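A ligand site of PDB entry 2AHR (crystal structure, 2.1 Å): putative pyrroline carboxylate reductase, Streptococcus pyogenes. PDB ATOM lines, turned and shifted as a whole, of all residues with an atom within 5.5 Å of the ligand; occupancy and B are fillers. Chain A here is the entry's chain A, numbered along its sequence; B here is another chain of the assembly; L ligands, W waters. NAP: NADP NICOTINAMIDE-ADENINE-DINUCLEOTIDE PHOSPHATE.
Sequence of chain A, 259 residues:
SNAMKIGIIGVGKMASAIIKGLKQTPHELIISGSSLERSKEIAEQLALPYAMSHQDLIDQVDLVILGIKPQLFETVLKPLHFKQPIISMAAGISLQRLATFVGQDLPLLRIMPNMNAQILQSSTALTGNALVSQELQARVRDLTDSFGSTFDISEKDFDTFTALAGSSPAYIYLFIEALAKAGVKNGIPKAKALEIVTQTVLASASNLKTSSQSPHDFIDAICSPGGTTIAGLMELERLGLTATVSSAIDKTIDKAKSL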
ATOM      1  N   ILE A   9     -26.631  -1.221  28.585  1.00  0.00           N
ATOM      2  CA  ILE A   9     -27.966  -1.760  28.416  1.00  0.00           C
ATOM      3  C   ILE A   9     -28.575  -1.230  27.134  1.00  0.00           C
ATOM      4  O   ILE A   9     -28.868  -0.020  27.015  1.00  0.00           O
ATOM      5  CB  ILE A   9     -28.908  -1.428  29.612  1.00  0.00           C
ATOM      6  CG1 ILE A   9     -28.295  -1.884  30.938  1.00  0.00           C
ATOM      7  CG2 ILE A   9     -30.309  -2.027  29.382  1.00  0.00           C
ATOM      8  CD1 ILE A   9     -29.115  -1.524  32.166  1.00  0.00           C
ATOM      9  N   GLY A  10     -28.831  -2.153  26.200  1.00  0.00           N
ATOM     10  CA  GLY A  10     -29.315  -1.805  24.878  1.00  0.00           C
ATOM     11  C   GLY A  10     -28.118  -1.509  23.988  1.00  0.00           C
ATOM     12  O   GLY A  10     -27.354  -0.579  24.249  1.00  0.00           O
ATOM     13  N   VAL A  11     -27.954  -2.327  22.951  1.00  0.00           N
ATOM     14  CA  VAL A  11     -26.804  -2.222  22.044  1.00  0.00           C
ATOM     15  C   VAL A  11     -27.271  -2.322  20.597  1.00  0.00           C
ATOM     16  O   VAL A  11     -27.369  -3.420  20.030  1.00  0.00           O
ATOM     17  CB  VAL A  11     -25.720  -3.279  22.354  1.00  0.00           C
ATOM     18  CG1 VAL A  11     -24.470  -2.993  21.574  1.00  0.00           C
ATOM     19  CG2 VAL A  11     -25.420  -3.307  23.829  1.00  0.00           C
ATOM     20  N   GLY A  12     -27.560  -1.168  20.022  1.00  0.00           N
ATOM     21  CA  GLY A  12     -27.964  -1.060  18.620  1.00  0.00           C
ATOM     22  C   GLY A  12     -26.836  -0.407  17.856  1.00  0.00           C
ATOM     23  O   GLY A  12     -25.669  -0.653  18.153  1.00  0.00           O
ATOM     24  N   LYS A  13     -27.204   0.436  16.892  1.00  0.00           N
ATOM     25  CA  LYS A  13     -26.208   1.061  15.995  1.00  0.00           C
ATOM     26  C   LYS A  13     -25.221   1.966  16.769  1.00  0.00           C
ATOM     27  O   LYS A  13     -24.005   1.741  16.749  1.00  0.00           O
ATOM     28  CB  LYS A  13     -26.864   1.851  14.851  1.00  0.00           C
ATOM     29  CG  LYS A  13     -27.914   1.111  13.981  1.00  0.00           C
ATOM     30  CD  LYS A  13     -27.368  -0.153  13.284  1.00  0.00           C
ATOM     31  CE  LYS A  13     -26.270   0.139  12.263  1.00  0.00           C
ATOM     32  NZ  LYS A  13     -25.969  -1.026  11.370  1.00  0.00           N
ATOM     33  N   MET A  14     -25.767   2.961  17.471  1.00  0.00           N
ATOM     34  CA  MET A  14     -24.952   3.926  18.213  1.00  0.00           C
ATOM     35  C   MET A  14     -24.088   3.244  19.293  1.00  0.00           C
ATOM     36  O   MET A  14     -22.865   3.422  19.322  1.00  0.00           O
ATOM     37  CB  MET A  14     -25.848   5.030  18.814  1.00  0.00           C
ATOM     38  CG  MET A  14     -25.187   6.423  19.021  1.00  0.00           C
ATOM     39  SD  MET A  14     -24.150   7.052  17.672  1.00  0.00           S
ATOM     40  CE  MET A  14     -22.563   6.441  18.194  1.00  0.00           C
ATOM     41  N   ALA A  15     -24.710   2.433  20.150  1.00  0.00           N
ATOM     42  CA  ALA A  15     -23.974   1.715  21.196  1.00  0.00           C
ATOM     43  C   ALA A  15     -22.838   0.830  20.641  1.00  0.00           C
ATOM     44  O   ALA A  15     -21.741   0.828  21.187  1.00  0.00           O
ATOM     45  CB  ALA A  15     -24.915   0.909  22.056  1.00  0.00           C
ATOM     46  N   SER A  32     -25.936  -5.999  27.816  1.00  0.00           N
ATOM     47  CA  SER A  32     -27.239  -6.633  28.011  1.00  0.00           C
ATOM     48  C   SER A  32     -28.257  -6.082  27.020  1.00  0.00           C
ATOM     49  O   SER A  32     -28.495  -4.875  26.990  1.00  0.00           O
ATOM     50  CB  SER A  32     -27.699  -6.402  29.465  1.00  0.00           C
ATOM     51  OG  SER A  32     -28.950  -6.991  29.726  1.00  0.00           O
ATOM     52  N   GLY A  33     -28.865  -6.966  26.225  1.00  0.00           N
ATOM     53  CA  GLY A  33     -29.798  -6.604  25.144  1.00  0.00           C
ATOM     54  C   GLY A  33     -31.285  -6.709  25.434  1.00  0.00           C
ATOM     55  O   GLY A  33     -31.691  -6.734  26.589  1.00  0.00           O
ATOM     56  N   SER A  34     -32.098  -6.775  24.380  1.00  0.00           N
ATOM     57  CA  SER A  34     -33.577  -6.828  24.476  1.00  0.00           C
ATOM     58  C   SER A  34     -34.170  -8.190  24.888  1.00  0.00           C
ATOM     59  O   SER A  34     -35.367  -8.287  25.207  1.00  0.00           O
ATOM     60  CB  SER A  34     -34.217  -6.403  23.151  1.00  0.00           C
ATOM     61  OG  SER A  34     -34.012  -7.371  22.135  1.00  0.00           O
ATOM     62  N   ARG A  38     -30.894 -12.321  22.037  1.00  0.00           N
ATOM     63  CA  ARG A  38     -30.303 -11.135  21.410  1.00  0.00           C
ATOM     64  C   ARG A  38     -29.028 -10.740  22.113  1.00  0.00           C
ATOM     65  O   ARG A  38     -28.051 -10.394  21.464  1.00  0.00           O
ATOM     66  CB  ARG A  38     -31.288  -9.964  21.414  1.00  0.00           C
ATOM     67  CG  ARG A  38     -32.463 -10.090  20.421  1.00  0.00           C
ATOM     68  CD  ARG A  38     -32.040  -9.961  18.967  1.00  0.00           C
ATOM     69  NE  ARG A  38     -31.568  -8.626  18.644  1.00  0.00           N
ATOM     70  CZ  ARG A  38     -30.393  -8.334  18.072  1.00  0.00           C
ATOM     71  NH1 ARG A  38     -30.074  -7.057  17.848  1.00  0.00           N
ATOM     72  NH2 ARG A  38     -29.549  -9.293  17.707  1.00  0.00           N
ATOM     73  N   ILE A  42     -25.435 -10.633  20.069  1.00  0.00           N
ATOM     74  CA  ILE A  42     -24.655  -9.396  20.081  1.00  0.00           C
ATOM     75  C   ILE A  42     -23.300  -9.556  20.776  1.00  0.00           C
ATOM     76  O   ILE A  42     -22.276  -9.052  20.296  1.00  0.00           O
ATOM     77  CB  ILE A  42     -25.462  -8.231  20.731  1.00  0.00           C
ATOM     78  CG1 ILE A  42     -26.681  -7.876  19.863  1.00  0.00           C
ATOM     79  CG2 ILE A  42     -24.570  -7.007  20.933  1.00  0.00           C
ATOM     80  CD1 ILE A  42     -27.775  -7.042  20.568  1.00  0.00           C
ATOM     81  N   HIS A  54     -30.974  -7.373  33.040  1.00  0.00           N
ATOM     82  CA  HIS A  54     -30.478  -6.013  33.296  1.00  0.00           C
ATOM     83  C   HIS A  54     -30.042  -5.824  34.738  1.00  0.00           C
ATOM     84  O   HIS A  54     -28.996  -5.229  34.999  1.00  0.00           O
ATOM     85  CB  HIS A  54     -31.477  -4.925  32.892  1.00  0.00           C
ATOM     86  CG  HIS A  54     -31.793  -4.890  31.432  1.00  0.00           C
ATOM     87  ND1 HIS A  54     -30.908  -5.341  30.474  1.00  0.00           N
ATOM     88  CD2 HIS A  54     -32.883  -4.447  30.760  1.00  0.00           C
ATOM     89  CE1 HIS A  54     -31.450  -5.205  29.273  1.00  0.00           C
ATOM     90  NE2 HIS A  54     -32.644  -4.664  29.417  1.00  0.00           N
ATOM     91  N   GLY A  67     -28.054   2.463  26.077  1.00  0.00           N
ATOM     92  CA  GLY A  67     -28.121   2.472  24.606  1.00  0.00           C
ATOM     93  C   GLY A  67     -29.479   2.222  23.962  1.00  0.00           C
ATOM     94  O   GLY A  67     -29.566   1.989  22.750  1.00  0.00           O
ATOM     95  N   ILE A  68     -30.536   2.298  24.765  1.00  0.00           N
ATOM     96  CA  ILE A  68     -31.904   2.085  24.279  1.00  0.00           C
ATOM     97  C   ILE A  68     -32.442   3.409  23.745  1.00  0.00           C
ATOM     98  O   ILE A  68     -31.895   4.476  24.039  1.00  0.00           O
ATOM     99  CB  ILE A  68     -32.857   1.520  25.380  1.00  0.00           C
ATOM    100  CG1 ILE A  68     -32.966   2.480  26.569  1.00  0.00           C
ATOM    101  CG2 ILE A  68     -32.396   0.134  25.838  1.00  0.00           C
ATOM    102  CD1 ILE A  68     -34.161   2.231  27.513  1.00  0.00           C
ATOM    103  N   LYS A  69     -33.515   3.340  22.949  1.00  0.00           N
ATOM    104  CA  LYS A  69     -34.191   4.531  22.432  1.00  0.00           C
ATOM    105  C   LYS A  69     -34.941   5.288  23.530  1.00  0.00           C
ATOM    106  O   LYS A  69     -35.426   4.675  24.498  1.00  0.00           O
ATOM    107  CB  LYS A  69     -35.143   4.155  21.303  1.00  0.00           C
ATOM    108  CG  LYS A  69     -34.462   3.769  19.992  1.00  0.00           C
ATOM    109  CD  LYS A  69     -35.460   3.748  18.814  1.00  0.00           C
ATOM    110  CE  LYS A  69     -36.453   2.551  18.850  1.00  0.00           C
ATOM    111  NZ  LYS A  69     -37.610   2.719  19.803  1.00  0.00           N
ATOM    112  N   PRO A  70     -35.034   6.623  23.398  1.00  0.00           N
ATOM    113  CA  PRO A  70     -35.685   7.443  24.428  1.00  0.00           C
ATOM    114  C   PRO A  70     -37.098   6.952  24.802  1.00  0.00           C
ATOM    115  O   PRO A  70     -37.436   6.893  25.987  1.00  0.00           O
ATOM    116  CB  PRO A  70     -35.756   8.857  23.813  1.00  0.00           C
ATOM    117  CG  PRO A  70     -35.322   8.723  22.356  1.00  0.00           C
ATOM    118  CD  PRO A  70     -34.521   7.429  22.274  1.00  0.00           C
ATOM    119  N   LEU A  72     -38.339   4.229  25.077  1.00  0.00           N
ATOM    120  CA  LEU A  72     -38.319   3.030  25.907  1.00  0.00           C
ATOM    121  C   LEU A  72     -37.761   3.271  27.303  1.00  0.00           C
ATOM    122  O   LEU A  72     -37.708   2.342  28.087  1.00  0.00           O
ATOM    123  CB  LEU A  72     -37.499   1.928  25.228  1.00  0.00           C
ATOM    124  CG  LEU A  72     -38.275   0.912  24.396  1.00  0.00           C
ATOM    125  CD1 LEU A  72     -38.993   1.544  23.207  1.00  0.00           C
ATOM    126  CD2 LEU A  72     -37.321  -0.157  23.917  1.00  0.00           C
ATOM    127  N   PHE A  73     -37.338   4.491  27.606  1.00  0.00           N
ATOM    128  CA  PHE A  73     -36.701   4.782  28.895  1.00  0.00           C
ATOM    129  C   PHE A  73     -37.579   4.396  30.112  1.00  0.00           C
ATOM    130  O   PHE A  73     -37.142   3.653  30.995  1.00  0.00           O
ATOM    131  CB  PHE A  73     -36.264   6.253  28.969  1.00  0.00           C
ATOM    132  CG  PHE A  73     -34.794   6.482  28.648  1.00  0.00           C
ATOM    133  CD1 PHE A  73     -34.213   5.927  27.505  1.00  0.00           C
ATOM    134  CD2 PHE A  73     -34.010   7.293  29.466  1.00  0.00           C
ATOM    135  CE1 PHE A  73     -32.854   6.140  27.211  1.00  0.00           C
ATOM    136  CE2 PHE A  73     -32.667   7.527  29.187  1.00  0.00           C
ATOM    137  CZ  PHE A  73     -32.085   6.929  28.056  1.00  0.00           C
ATOM    138  N   VAL A  76     -38.440   0.453  30.326  1.00  0.00           N
ATOM    139  CA  VAL A  76     -37.282  -0.409  30.567  1.00  0.00           C
ATOM    140  C   VAL A  76     -36.552  -0.092  31.885  1.00  0.00           C
ATOM    141  O   VAL A  76     -36.011  -0.989  32.521  1.00  0.00           O
ATOM    142  CB  VAL A  76     -36.277  -0.366  29.335  1.00  0.00           C
ATOM    143  CG1 VAL A  76     -34.999  -1.136  29.615  1.00  0.00           C
ATOM    144  CG2 VAL A  76     -36.946  -0.901  28.081  1.00  0.00           C
ATOM    145  N   MET A  89     -27.095   8.196  26.340  1.00  0.00           N
ATOM    146  CA  MET A  89     -26.778   8.763  25.004  1.00  0.00           C
ATOM    147  C   MET A  89     -28.042   9.233  24.245  1.00  0.00           C
ATOM    148  O   MET A  89     -27.972   9.659  23.088  1.00  0.00           O
ATOM    149  CB  MET A  89     -25.946   7.794  24.154  1.00  0.00           C
ATOM    150  CG  MET A  89     -26.727   6.642  23.442  1.00  0.00           C
ATOM    151  SD  MET A  89     -25.725   5.335  22.618  1.00  0.00           S
ATOM    152  CE  MET A  89     -24.477   5.064  23.857  1.00  0.00           C
ATOM    153  N   ALA A  90     -29.187   9.171  24.913  1.00  0.00           N
ATOM    154  CA  ALA A  90     -30.481   9.383  24.277  1.00  0.00           C
ATOM    155  C   ALA A  90     -30.806  10.835  23.986  1.00  0.00           C
ATOM    156  O   ALA A  90     -30.655  11.701  24.854  1.00  0.00           O
ATOM    157  CB  ALA A  90     -31.566   8.798  25.135  1.00  0.00           C
ATOM    158  N   ALA A  91     -31.285  11.083  22.767  1.00  0.00           N
ATOM    159  CA  ALA A  91     -31.861  12.369  22.369  1.00  0.00           C
ATOM    160  C   ALA A  91     -33.122  12.654  23.187  1.00  0.00           C
ATOM    161  O   ALA A  91     -33.858  11.742  23.516  1.00  0.00           O
ATOM    162  CB  ALA A  91     -32.214  12.363  20.883  1.00  0.00           C
ATOM    163  N   MET A 112     -23.937  13.086  23.825  1.00  0.00           N
ATOM    164  CA  MET A 112     -24.527  13.075  22.509  1.00  0.00           C
ATOM    165  C   MET A 112     -23.431  12.833  21.486  1.00  0.00           C
ATOM    166  O   MET A 112     -22.764  13.781  21.039  1.00  0.00           O
ATOM    167  CB  MET A 112     -25.327  14.359  22.198  1.00  0.00           C
ATOM    168  CG  MET A 112     -25.965  14.365  20.773  1.00  0.00           C
ATOM    169  SD  MET A 112     -26.939  12.899  20.343  1.00  0.00           S
ATOM    170  CE  MET A 112     -28.068  12.847  21.738  1.00  0.00           C
ATOM    171  N   PRO A 113     -23.193  11.547  21.146  1.00  0.00           N
ATOM    172  CA  PRO A 113     -22.215  11.153  20.152  1.00  0.00           C
ATOM    173  C   PRO A 113     -22.823  11.120  18.741  1.00  0.00           C
ATOM    174  O   PRO A 113     -24.005  11.484  18.554  1.00  0.00           O
ATOM    175  CB  PRO A 113     -21.851   9.720  20.580  1.00  0.00           C
ATOM    176  CG  PRO A 113     -23.165   9.174  21.064  1.00  0.00           C
ATOM    177  CD  PRO A 113     -23.876  10.364  21.733  1.00  0.00           C
ATOM    178  N   ASN A 114     -22.039  10.686  17.760  1.00  0.00           N
ATOM    179  CA  ASN A 114     -22.570  10.431  16.430  1.00  0.00           C
ATOM    180  C   ASN A 114     -21.904   9.219  15.818  1.00  0.00           C
ATOM    181  O   ASN A 114     -20.964   8.678  16.415  1.00  0.00           O
ATOM    182  CB  ASN A 114     -22.453  11.675  15.540  1.00  0.00           C
ATOM    183  CG  ASN A 114     -21.010  12.059  15.236  1.00  0.00           C
ATOM    184  OD1 ASN A 114     -20.135  11.197  15.112  1.00  0.00           O
ATOM    185  ND2 ASN A 114     -20.762  13.349  15.100  1.00  0.00           N
ATOM    186  N   MET A 115     -22.354   8.795  14.636  1.00  0.00           N
ATOM    187  CA  MET A 115     -21.947   7.516  14.031  1.00  0.00           C
ATOM    188  C   MET A 115     -20.435   7.436  13.701  1.00  0.00           C
ATOM    189  O   MET A 115     -19.887   6.341  13.449  1.00  0.00           O
ATOM    190  CB  MET A 115     -22.807   7.212  12.776  1.00  0.00           C
ATOM    191  CG  MET A 115     -22.885   5.706  12.368  1.00  0.00           C
ATOM    192  SD  MET A 115     -23.412   4.487  13.624  1.00  0.00           S
ATOM    193  CE  MET A 115     -25.060   5.067  14.071  1.00  0.00           C
ATOM    194  N   GLY A 166     -25.077  15.170  16.079  1.00  0.00           N
ATOM    195  CA  GLY A 166     -25.666  13.823  16.176  1.00  0.00           C
ATOM    196  C   GLY A 166     -26.473  13.405  14.957  1.00  0.00           C
ATOM    197  O   GLY A 166     -26.287  12.294  14.417  1.00  0.00           O
ATOM    198  N   ALA B 221     -28.690   3.852   9.132  1.00  0.00           N
ATOM    199  CA  ALA B 221     -28.069   3.602  10.435  1.00  0.00           C
ATOM    200  C   ALA B 221     -28.346   4.739  11.405  1.00  0.00           C
ATOM    201  O   ALA B 221     -28.695   4.520  12.556  1.00  0.00           O
ATOM    202  CB  ALA B 221     -26.546   3.356  10.288  1.00  0.00           C
ATOM    203  N   ILE B 222     -28.211   5.960  10.927  1.00  0.00           N
ATOM    204  CA  ILE B 222     -28.332   7.153  11.756  1.00  0.00           C
ATOM    205  C   ILE B 222     -29.806   7.483  12.142  1.00  0.00           C
ATOM    206  O   ILE B 222     -30.065   8.079  13.207  1.00  0.00           O
ATOM    207  CB  ILE B 222     -27.604   8.340  11.047  1.00  0.00           C
ATOM    208  CG1 ILE B 222     -26.079   8.079  10.988  1.00  0.00           C
ATOM    209  CG2 ILE B 222     -27.879   9.688  11.740  1.00  0.00           C
ATOM    210  CD1 ILE B 222     -25.355   8.715   9.786  1.00  0.00           C
ATOM    211  N   CYS B 223     -30.755   7.082  11.298  1.00  0.00           N
ATOM    212  CA  CYS B 223     -32.187   7.399  11.538  1.00  0.00           C
ATOM    213  C   CYS B 223     -32.878   6.425  12.510  1.00  0.00           C
ATOM    214  O   CYS B 223     -33.570   5.491  12.084  1.00  0.00           O
ATOM    215  CB  CYS B 223     -32.951   7.434  10.198  1.00  0.00           C
ATOM    216  SG  CYS B 223     -32.619   8.890   9.179  1.00  0.00           S
ATOM    217  N   SER B 224     -32.700   6.624  13.829  1.00  0.00           N
ATOM    218  CA  SER B 224     -33.392   5.786  14.820  1.00  0.00           C
ATOM    219  C   SER B 224     -34.897   5.939  14.595  1.00  0.00           C
ATOM    220  O   SER B 224     -35.364   7.054  14.368  1.00  0.00           O
ATOM    221  CB  SER B 224     -33.076   6.233  16.249  1.00  0.00           C
ATOM    222  OG  SER B 224     -31.768   6.730  16.364  1.00  0.00           O
ATOM    223  N   PRO B 225     -35.663   4.830  14.674  1.00  0.00           N
ATOM    224  CA  PRO B 225     -37.115   4.908  14.529  1.00  0.00           C
ATOM    225  C   PRO B 225     -37.763   5.915  15.481  1.00  0.00           C
ATOM    226  O   PRO B 225     -37.406   5.959  16.662  1.00  0.00           O
ATOM    227  CB  PRO B 225     -37.574   3.488  14.847  1.00  0.00           C
ATOM    228  CG  PRO B 225     -36.369   2.620  14.573  1.00  0.00           C
ATOM    229  CD  PRO B 225     -35.183   3.452  14.890  1.00  0.00           C
HETATM  230  PA  NAP L   1     -31.292   1.139  17.633  1.00  0.00           P
HETATM  231  O1A NAP L   1     -32.678   0.819  17.163  1.00  0.00           O
HETATM  232  O2A NAP L   1     -30.214   0.702  16.705  1.00  0.00           O
HETATM  233  O5B NAP L   1     -30.948   0.479  19.063  1.00  0.00           O
HETATM  234  C5B NAP L   1     -31.911   0.226  20.044  1.00  0.00           C
HETATM  235  C4B NAP L   1     -31.494  -1.065  20.721  1.00  0.00           C
HETATM  236  O4B NAP L   1     -32.175  -1.240  21.944  1.00  0.00           O
HETATM  237  C3B NAP L   1     -31.825  -2.264  19.825  1.00  0.00           C
HETATM  238  O3B NAP L   1     -30.632  -2.993  19.630  1.00  0.00           O
HETATM  239  C2B NAP L   1     -32.851  -3.054  20.625  1.00  0.00           C
HETATM  240  O2B NAP L   1     -32.715  -4.469  20.538  1.00  0.00           O
HETATM  241  C1B NAP L   1     -32.556  -2.588  22.044  1.00  0.00           C
HETATM  242  N9A NAP L   1     -33.680  -2.832  22.966  1.00  0.00           N
HETATM  243  C8A NAP L   1     -35.035  -2.846  22.678  1.00  0.00           C
HETATM  244  N7A NAP L   1     -35.691  -3.158  23.828  1.00  0.00           N
HETATM  245  C5A NAP L   1     -34.778  -3.364  24.821  1.00  0.00           C
HETATM  246  C6A NAP L   1     -34.898  -3.697  26.173  1.00  0.00           C
HETATM  247  N6A NAP L   1     -36.083  -4.089  26.634  1.00  0.00           N
HETATM  248  N1A NAP L   1     -33.774  -3.830  26.962  1.00  0.00           N
HETATM  249  C2A NAP L   1     -32.524  -3.623  26.403  1.00  0.00           C
HETATM  250  N3A NAP L   1     -32.390  -3.302  25.057  1.00  0.00           N
HETATM  251  C4A NAP L   1     -33.511  -3.153  24.291  1.00  0.00           C
HETATM  252  O3  NAP L   1     -31.254   2.723  17.967  1.00  0.00           O
HETATM  253  PN  NAP L   1     -29.937   3.671  17.881  1.00  0.00           P
HETATM  254  O1N NAP L   1     -30.090   4.424  16.609  1.00  0.00           O
HETATM  255  O2N NAP L   1     -28.688   2.926  18.148  1.00  0.00           O
HETATM  256  O5D NAP L   1     -30.196   4.690  19.112  1.00  0.00           O
HETATM  257  C5D NAP L   1     -29.742   4.424  20.408  1.00  0.00           C
HETATM  258  C4D NAP L   1     -29.742   5.699  21.223  1.00  0.00           C
HETATM  259  O4D NAP L   1     -28.691   6.550  20.793  1.00  0.00           O
HETATM  260  C3D NAP L   1     -31.023   6.505  21.083  1.00  0.00           C
HETATM  261  O3D NAP L   1     -31.396   6.829  22.399  1.00  0.00           O
HETATM  262  C2D NAP L   1     -30.682   7.746  20.247  1.00  0.00           C
HETATM  263  O2D NAP L   1     -31.438   8.892  20.625  1.00  0.00           O
HETATM  264  C1D NAP L   1     -29.161   7.859  20.485  1.00  0.00           C
HETATM  265  N1N NAP L   1     -28.346   8.322  19.337  1.00  0.00           N
HETATM  266  C2N NAP L   1     -28.432   7.662  18.133  1.00  0.00           C
HETATM  267  C3N NAP L   1     -27.641   8.084  17.052  1.00  0.00           C
HETATM  268  C7N NAP L   1     -27.639   7.321  15.768  1.00  0.00           C
HETATM  269  O7N NAP L   1     -26.876   7.851  14.738  1.00  0.00           O
HETATM  270  N7N NAP L   1     -28.308   6.172  15.618  1.00  0.00           N
HETATM  271  C4N NAP L   1     -26.772   9.169  17.225  1.00  0.00           C
HETATM  272  C5N NAP L   1     -26.706   9.835  18.453  1.00  0.00           C
HETATM  273  C6N NAP L   1     -27.493   9.391  19.514  1.00  0.00           C
HETATM  274  P2B NAP L   1     -33.201  -5.274  19.228  1.00  0.00           P
HETATM  275  O1X NAP L   1     -33.292  -6.750  19.556  1.00  0.00           O
HETATM  276  O2X NAP L   1     -34.581  -4.778  18.832  1.00  0.00           O
HETATM  277  O3X NAP L   1     -32.178  -5.066  18.121  1.00  0.00           O
HETATM  278  O   HOH W   1     -36.090  -0.704  20.318  1.00  0.00           O
HETATM  279  O   HOH W   2     -33.788   8.922  19.399  1.00  0.00           O
HETATM  280  O   HOH W   3     -34.320   0.544  22.280  1.00  0.00           O
HETATM  281  O   HOH W   4     -27.646   1.649  20.594  1.00  0.00           O
HETATM  282  O   HOH W   5     -31.194  -6.687  21.761  1.00  0.00           O
HETATM  283  O   HOH W   6     -29.792  -4.434  21.588  1.00  0.00           O
HETATM  284  O   HOH W   7     -29.669  -2.078  15.568  1.00  0.00           O
HETATM  285  O   HOH W   8     -37.376  -5.180  20.161  1.00  0.00           O
HETATM  286  O   HOH W   9     -24.952   9.888  14.176  1.00  0.00           O
HETATM  287  O   HOH W  10     -30.731   3.515  13.988  1.00  0.00           O
HETATM  288  O   HOH W  11     -31.646  -3.534  15.944  1.00  0.00           O
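The side-chain hydroxyl (OG) of Ser 32 is in hydrogen-bond range of a ring nitrogen (ND1) of His 54, 2.7 Å away.
N of Gly 67 is in hydrogen-bond range of O of Ile 9 (2.8 Å).
The backbone carbonyl oxygen of Ser 32 is in hydrogen-bond range of the backbone NH of Gly 10 (2.9 Å).
The side-chain sulfur (SD) of Met 89 lies close to an oxygen (O4D) of the ligand.
Merely in contact with the ligand: Gly 10, Gly 12, Gly 33, Gly 67, Lys 69, Pro 70, Leu 72, Val 76, Ala 90, Met 112, Pro 113, Met 115, Ala 221 of chain B and Ile 222 of chain B.
Hydrophobic or aromatic side chains within 4 Å of the ligand: Met 14, His 54, Ile 68, Pro 70, Leu 72, Val 76, Met 89, Ala 90, Ala 91, Met 112, Met 115 and Ile 222 of chain B.
Within 4 Å of the ligand: Gly 10, Val 11, Gly 12, Lys 13, Met 14, Gly 33, Ser 34, Arg 38, His 54, Gly 67, Ile 68, Lys 69, Pro 70, Leu 72, Val 76, Met 89, Ala 90, Ala 91, Met 112, Pro 113, Met 115, Ala 221 of chain B, Ile 222 of chain B and Ser 224 of chain B.
Water W6 lies within hydrogen-bond range of an oxygen (O3B) of the ligand (2.6 Å) and the backbone carbonyl oxygen of Val 11 (3.1 Å).
Water W3 lies within hydrogen-bond range of an oxygen (O4B) of the ligand and the backbone NH (N) of Lys 69.
Water W10 bridges the backbone carbonyl oxygen of Ala 221 of chain B (2.7 Å) and an oxygen (O1N) of the ligand (2.8 Å).
Water W9 lies within hydrogen-bond range of the backbone carbonyl oxygen of Gly 166 (2.8 Å), the backbone NH of Met 115 (2.9 Å) and an oxygen (O7N) of the ligand (2.9 Å).
Water W4 lies within hydrogen-bond range of N of Gly 12, O of Gly 67, O2N of the ligand and N of Ala 15.
Water W5 bridges N of Ser 34 (2.8 Å) and O2B of the ligand (3.0 Å).
The guanidinium group (NE) of Arg 38 is in salt-bridge range of an oxygen (O1X) of the ligand (2.7 Å).
The side-chain hydroxyl (OG) of Ser 34 sits at hydrogen-bond distance from an oxygen (O1X) of the ligand (2.7 Å).
A nitrogen (N1A) of the ligand is in hydrogen-bond range of a ring nitrogen (NE2) of His 54 (2.8 Å).
OG of Ser 224 of chain B lies within hydrogen-bond range of O1N of the ligand (2.9 Å).
O3D of the ligand is in hydrogen-bond range of O of Ile 68 (2.9 Å).
An oxygen (O2N) of the ligand sits at hydrogen-bond distance from the backbone NH of Met 14 (3.0 Å).
N of Lys 13 is in hydrogen-bond range of O2A of the ligand, at 3.0 Å.
N of Ala 91 is in hydrogen-bond range of O2D of the ligand, 3.1 Å away.
An oxygen (O3B) of the ligand sits at hydrogen-bond distance from the backbone carbonyl oxygen (O) of Val 11, at 3.3 Å.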
